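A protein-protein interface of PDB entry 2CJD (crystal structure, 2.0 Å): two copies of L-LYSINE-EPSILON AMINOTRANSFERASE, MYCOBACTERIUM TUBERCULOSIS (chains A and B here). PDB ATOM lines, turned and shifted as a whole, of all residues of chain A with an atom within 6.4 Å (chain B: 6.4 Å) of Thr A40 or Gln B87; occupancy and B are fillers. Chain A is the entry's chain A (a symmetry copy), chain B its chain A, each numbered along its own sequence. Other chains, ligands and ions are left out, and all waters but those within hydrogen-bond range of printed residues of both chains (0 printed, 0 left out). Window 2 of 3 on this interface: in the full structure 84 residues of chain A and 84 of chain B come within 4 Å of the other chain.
N of Thr A40 sits at hydrogen-bond distance from OD1 of Asp A38 (3.0 Å).
The backbone carbonyl oxygen (O) of Leu A39 lies within hydrogen-bond range of the side-chain amide nitrogen (ND2) of Asn A71, 2.8 Å away.
The backbone carbonyl oxygen of Ser A42 lies within hydrogen-bond range of the side-chain amide nitrogen of Asn A71, 2.9 Å away.
No position is printed for both chains.
Of the 3 pairs that touch across the chains among the printed residues, none has its exchanged pair printed and touching as well.
Among the printed residues, merely in contact across the chains: Thr A40 with Gln B87 and Met A70 with Asn B91.
Thr A40 touches one residue of chain B.
Printed residues of chain B within 4 Å of Met A70: Asn B91 (3.7 Å).
Of the printed residues of chain B, Asn A71 touches Asn B91 (2.8 Å).
Of chain A, only Thr A40 (3.6 Å) comes within 4 Å of Gln B87.
Of the printed residues of chain A, Asn B91 touches Met A70 (3.7 Å) and Asn A71 (2.8 Å).
The nearest printed residue of chain A that does not touch Asn B91 is Leu A39 (4.3 Å).
Of the 9 printed residues of chain A, 3 touch a printed residue of chain B.
Along chain A the printed residues that touch a printed residue of chain B span positions 40 to 71.
OD1 of Asn B91 sits at hydrogen-bond distance from N of Asn A71, 2.8 Å away.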
ATOM      1  N   LEU A  37      -1.448  14.085  21.688  1.00  0.00           N
ATOM      2  CA  LEU A  37      -2.685  14.395  22.384  1.00  0.00           C
ATOM      3  C   LEU A  37      -3.720  13.283  22.247  1.00  0.00           C
ATOM      4  O   LEU A  37      -4.149  12.949  21.151  1.00  0.00           O
ATOM      5  CB  LEU A  37      -3.337  15.682  21.835  1.00  0.00           C
ATOM      6  CG  LEU A  37      -4.107  16.673  22.742  1.00  0.00           C
ATOM      7  CD1 LEU A  37      -5.350  17.300  22.096  1.00  0.00           C
ATOM      8  CD2 LEU A  37      -4.363  16.237  24.164  1.00  0.00           C
ATOM      9  N   ASP A  38      -4.178  12.781  23.383  1.00  0.00           N
ATOM     10  CA  ASP A  38      -5.319  11.903  23.409  1.00  0.00           C
ATOM     11  C   ASP A  38      -6.602  12.753  23.432  1.00  0.00           C
ATOM     12  O   ASP A  38      -6.911  13.354  24.451  1.00  0.00           O
ATOM     13  CB  ASP A  38      -5.252  11.009  24.641  1.00  0.00           C
ATOM     14  CG  ASP A  38      -6.290   9.899  24.613  1.00  0.00           C
ATOM     15  OD1 ASP A  38      -7.497  10.135  24.319  1.00  0.00           O
ATOM     16  OD2 ASP A  38      -5.877   8.768  24.886  1.00  0.00           O
ATOM     17  N   LEU A  39      -7.347  12.745  22.326  1.00  0.00           N
ATOM     18  CA  LEU A  39      -8.494  13.617  22.131  1.00  0.00           C
ATOM     19  C   LEU A  39      -9.657  13.204  22.997  1.00  0.00           C
ATOM     20  O   LEU A  39     -10.497  14.012  23.335  1.00  0.00           O
ATOM     21  CB  LEU A  39      -8.919  13.630  20.645  1.00  0.00           C
ATOM     22  CG  LEU A  39      -7.880  14.228  19.668  1.00  0.00           C
ATOM     23  CD1 LEU A  39      -8.446  14.168  18.233  1.00  0.00           C
ATOM     24  CD2 LEU A  39      -7.593  15.648  20.045  1.00  0.00           C
ATOM     25  N   THR A  40      -9.677  11.933  23.360  1.00  0.00           N
ATOM     26  CA  THR A  40     -10.778  11.367  24.116  1.00  0.00           C
ATOM     27  C   THR A  40     -10.596  11.409  25.638  1.00  0.00           C
ATOM     28  O   THR A  40     -11.538  11.718  26.365  1.00  0.00           O
ATOM     29  CB  THR A  40     -11.025   9.936  23.610  1.00  0.00           C
ATOM     30  OG1 THR A  40     -11.774  10.048  22.397  1.00  0.00           O
ATOM     31  CG2 THR A  40     -11.812   9.117  24.597  1.00  0.00           C
ATOM     32  N   ARG A  41      -9.395  11.099  26.106  1.00  0.00           N
ATOM     33  CA  ARG A  41      -9.125  10.950  27.531  1.00  0.00           C
ATOM     34  C   ARG A  41      -8.719  12.243  28.219  1.00  0.00           C
ATOM     35  O   ARG A  41      -8.840  12.346  29.450  1.00  0.00           O
ATOM     36  CB  ARG A  41      -8.128   9.808  27.788  1.00  0.00           C
ATOM     37  CG  ARG A  41      -8.718   8.482  27.369  1.00  0.00           C
ATOM     38  CD  ARG A  41      -7.795   7.298  27.675  1.00  0.00           C
ATOM     39  NE  ARG A  41      -7.803   6.353  26.555  1.00  0.00           N
ATOM     40  CZ  ARG A  41      -8.645   5.336  26.433  1.00  0.00           C
ATOM     41  NH1 ARG A  41      -9.551   5.102  27.378  1.00  0.00           N
ATOM     42  NH2 ARG A  41      -8.572   4.542  25.368  1.00  0.00           N
ATOM     43  N   SER A  42      -8.257  13.225  27.435  1.00  0.00           N
ATOM     44  CA  SER A  42      -7.985  14.575  27.960  1.00  0.00           C
ATOM     45  C   SER A  42      -9.266  15.210  28.498  1.00  0.00           C
ATOM     46  O   SER A  42     -10.365  14.932  28.004  1.00  0.00           O
ATOM     47  CB  SER A  42      -7.372  15.466  26.886  1.00  0.00           C
ATOM     48  OG  SER A  42      -6.143  14.910  26.465  1.00  0.00           O
ATOM     49  N   GLY A  43      -9.147  16.052  29.515  1.00  0.00           N
ATOM     50  CA  GLY A  43     -10.378  16.647  30.075  1.00  0.00           C
ATOM     51  C   GLY A  43     -10.089  17.686  31.118  1.00  0.00           C
ATOM     52  O   GLY A  43      -9.178  17.516  31.936  1.00  0.00           O
ATOM     53  N   MET A  70     -10.268  20.876  27.898  1.00  0.00           N
ATOM     54  CA  MET A  70     -10.619  19.764  27.007  1.00  0.00           C
ATOM     55  C   MET A  70     -11.921  19.072  27.395  1.00  0.00           C
ATOM     56  O   MET A  70     -12.210  18.856  28.580  1.00  0.00           O
ATOM     57  CB  MET A  70      -9.493  18.712  26.956  1.00  0.00           C
ATOM     58  CG  MET A  70      -8.293  19.107  26.099  1.00  0.00           C
ATOM     59  SD  MET A  70      -8.643  19.031  24.327  1.00  0.00           S
ATOM     60  CE  MET A  70      -8.705  17.279  23.970  1.00  0.00           C
ATOM     61  N   ASN A  71     -12.710  18.724  26.387  1.00  0.00           N
ATOM     62  CA  ASN A  71     -13.890  17.875  26.595  1.00  0.00           C
ATOM     63  C   ASN A  71     -14.735  18.305  27.799  1.00  0.00           C
ATOM     64  O   ASN A  71     -14.936  17.524  28.716  1.00  0.00           O
ATOM     65  CB  ASN A  71     -13.464  16.397  26.710  1.00  0.00           C
ATOM     66  CG  ASN A  71     -12.870  15.869  25.422  1.00  0.00           C
ATOM     67  OD1 ASN A  71     -13.402  16.127  24.343  1.00  0.00           O
ATOM     68  ND2 ASN A  71     -11.752  15.146  25.521  1.00  0.00           N
ATOM     69  N   HIS B  82     -18.020   9.153  11.875  1.00  0.00           N
ATOM     70  CA  HIS B  82     -18.792   9.983  12.811  1.00  0.00           C
ATOM     71  C   HIS B  82     -18.090  10.157  14.133  1.00  0.00           C
ATOM     72  O   HIS B  82     -17.971  11.268  14.610  1.00  0.00           O
ATOM     73  CB  HIS B  82     -20.177   9.431  13.063  1.00  0.00           C
ATOM     74  CG  HIS B  82     -21.072   9.519  11.878  1.00  0.00           C
ATOM     75  ND1 HIS B  82     -20.689  10.135  10.705  1.00  0.00           N
ATOM     76  CD2 HIS B  82     -22.341   9.094  11.686  1.00  0.00           C
ATOM     77  CE1 HIS B  82     -21.681  10.072   9.836  1.00  0.00           C
ATOM     78  NE2 HIS B  82     -22.699   9.453  10.407  1.00  0.00           N
ATOM     79  N   ALA B  83     -17.599   9.061  14.703  1.00  0.00           N
ATOM     80  CA  ALA B  83     -16.858   9.088  15.976  1.00  0.00           C
ATOM     81  C   ALA B  83     -15.544   9.864  15.874  1.00  0.00           C
ATOM     82  O   ALA B  83     -15.177  10.572  16.795  1.00  0.00           O
ATOM     83  CB  ALA B  83     -16.617   7.663  16.500  1.00  0.00           C
ATOM     84  N   GLU B  84     -14.832   9.725  14.766  1.00  0.00           N
ATOM     85  CA  GLU B  84     -13.576  10.446  14.566  1.00  0.00           C
ATOM     86  C   GLU B  84     -13.822  11.945  14.413  1.00  0.00           C
ATOM     87  O   GLU B  84     -13.127  12.762  15.019  1.00  0.00           O
ATOM     88  CB  GLU B  84     -12.830   9.900  13.342  1.00  0.00           C
ATOM     89  CG  GLU B  84     -12.457   8.413  13.505  1.00  0.00           C
ATOM     90  CD  GLU B  84     -12.002   7.744  12.214  1.00  0.00           C
ATOM     91  OE1 GLU B  84     -12.374   8.198  11.094  1.00  0.00           O
ATOM     92  OE2 GLU B  84     -11.272   6.734  12.342  1.00  0.00           O
ATOM     93  N   LEU B  85     -14.816  12.288  13.604  1.00  0.00           N
ATOM     94  CA  LEU B  85     -15.208  13.673  13.388  1.00  0.00           C
ATOM     95  C   LEU B  85     -15.669  14.338  14.695  1.00  0.00           C
ATOM     96  O   LEU B  85     -15.264  15.435  15.010  1.00  0.00           O
ATOM     97  CB  LEU B  85     -16.310  13.765  12.339  1.00  0.00           C
ATOM     98  CG  LEU B  85     -16.662  15.183  11.879  1.00  0.00           C
ATOM     99  CD1 LEU B  85     -15.466  15.870  11.206  1.00  0.00           C
ATOM    100  CD2 LEU B  85     -17.830  15.093  10.947  1.00  0.00           C
ATOM    101  N   MET B  86     -16.525  13.659  15.447  1.00  0.00           N
ATOM    102  CA  MET B  86     -16.998  14.170  16.724  1.00  0.00           C
ATOM    103  C   MET B  86     -15.843  14.440  17.717  1.00  0.00           C
ATOM    104  O   MET B  86     -15.792  15.503  18.368  1.00  0.00           O
ATOM    105  CB  MET B  86     -18.037  13.172  17.256  1.00  0.00           C
ATOM    106  CG  MET B  86     -18.720  13.508  18.560  1.00  0.00           C
ATOM    107  SD  MET B  86     -19.945  14.869  18.508  1.00  0.00           S
ATOM    108  CE  MET B  86     -20.024  15.396  16.801  1.00  0.00           C
ATOM    109  N   GLN B  87     -14.905  13.492  17.816  1.00  0.00           N
ATOM    110  CA  GLN B  87     -13.712  13.656  18.644  1.00  0.00           C
ATOM    111  C   GLN B  87     -12.948  14.902  18.254  1.00  0.00           C
ATOM    112  O   GLN B  87     -12.418  15.598  19.110  1.00  0.00           O
ATOM    113  CB  GLN B  87     -12.743  12.480  18.456  1.00  0.00           C
ATOM    114  CG  GLN B  87     -13.108  11.206  19.163  1.00  0.00           C
ATOM    115  CD  GLN B  87     -12.108  10.067  18.858  1.00  0.00           C
ATOM    116  OE1 GLN B  87     -12.516   8.893  18.731  1.00  0.00           O
ATOM    117  NE2 GLN B  87     -10.807  10.411  18.718  1.00  0.00           N
ATOM    118  N   ALA B  88     -12.838  15.150  16.948  1.00  0.00           N
ATOM    119  CA  ALA B  88     -12.118  16.329  16.477  1.00  0.00           C
ATOM    120  C   ALA B  88     -12.919  17.601  16.708  1.00  0.00           C
ATOM    121  O   ALA B  88     -12.338  18.620  17.095  1.00  0.00           O
ATOM    122  CB  ALA B  88     -11.752  16.178  15.011  1.00  0.00           C
ATOM    123  N   ALA B  89     -14.244  17.545  16.495  1.00  0.00           N
ATOM    124  CA  ALA B  89     -15.098  18.747  16.510  1.00  0.00           C
ATOM    125  C   ALA B  89     -15.352  19.337  17.906  1.00  0.00           C
ATOM    126  O   ALA B  89     -15.645  20.514  18.031  1.00  0.00           O
ATOM    127  CB  ALA B  89     -16.462  18.481  15.783  1.00  0.00           C
ATOM    128  N   LEU B  90     -15.242  18.517  18.948  1.00  0.00           N
ATOM    129  CA  LEU B  90     -15.546  18.964  20.297  1.00  0.00           C
ATOM    130  C   LEU B  90     -14.554  19.990  20.811  1.00  0.00           C
ATOM    131  O   LEU B  90     -14.920  20.865  21.594  1.00  0.00           O
ATOM    132  CB  LEU B  90     -15.630  17.774  21.266  1.00  0.00           C
ATOM    133  CG  LEU B  90     -16.967  17.014  21.206  1.00  0.00           C
ATOM    134  CD1 LEU B  90     -16.795  15.632  21.880  1.00  0.00           C
ATOM    135  CD2 LEU B  90     -18.095  17.798  21.900  1.00  0.00           C
ATOM    136  N   ASN B  91     -13.309  19.889  20.373  1.00  0.00           N
ATOM    137  CA  ASN B  91     -12.257  20.789  20.819  1.00  0.00           C
ATOM    138  C   ASN B  91     -11.588  21.439  19.619  1.00  0.00           C
ATOM    139  O   ASN B  91     -11.900  21.124  18.459  1.00  0.00           O
ATOM    140  CB  ASN B  91     -11.238  19.970  21.622  1.00  0.00           C
ATOM    141  CG  ASN B  91     -11.914  19.131  22.694  1.00  0.00           C
ATOM    142  OD1 ASN B  91     -12.349  19.658  23.734  1.00  0.00           O
ATOM    143  ND2 ASN B  91     -12.079  17.851  22.415  1.00  0.00           N
ATOM    144  N   ALA B 102      -5.182  11.963  14.611  1.00  0.00           N
ATOM    145  CA  ALA B 102      -6.113  12.544  13.638  1.00  0.00           C
ATOM    146  C   ALA B 102      -5.386  13.447  12.625  1.00  0.00           C
ATOM    147  O   ALA B 102      -5.606  13.355  11.408  1.00  0.00           O
ATOM    148  CB  ALA B 102      -7.205  13.321  14.371  1.00  0.00           C
ATOM    149  N   LEU B 335      -8.486  21.381  13.098  1.00  0.00           N
ATOM    150  CA  LEU B 335      -8.444  19.905  13.146  1.00  0.00           C
ATOM    151  C   LEU B 335      -9.720  19.240  12.584  1.00  0.00           C
ATOM    152  O   LEU B 335      -9.634  18.202  11.927  1.00  0.00           O
ATOM    153  CB  LEU B 335      -8.195  19.399  14.566  1.00  0.00           C
ATOM    154  CG  LEU B 335      -8.009  17.889  14.735  1.00  0.00           C
ATOM    155  CD1 LEU B 335      -6.713  17.451  13.963  1.00  0.00           C
ATOM    156  CD2 LEU B 335      -7.879  17.591  16.226  1.00  0.00           C
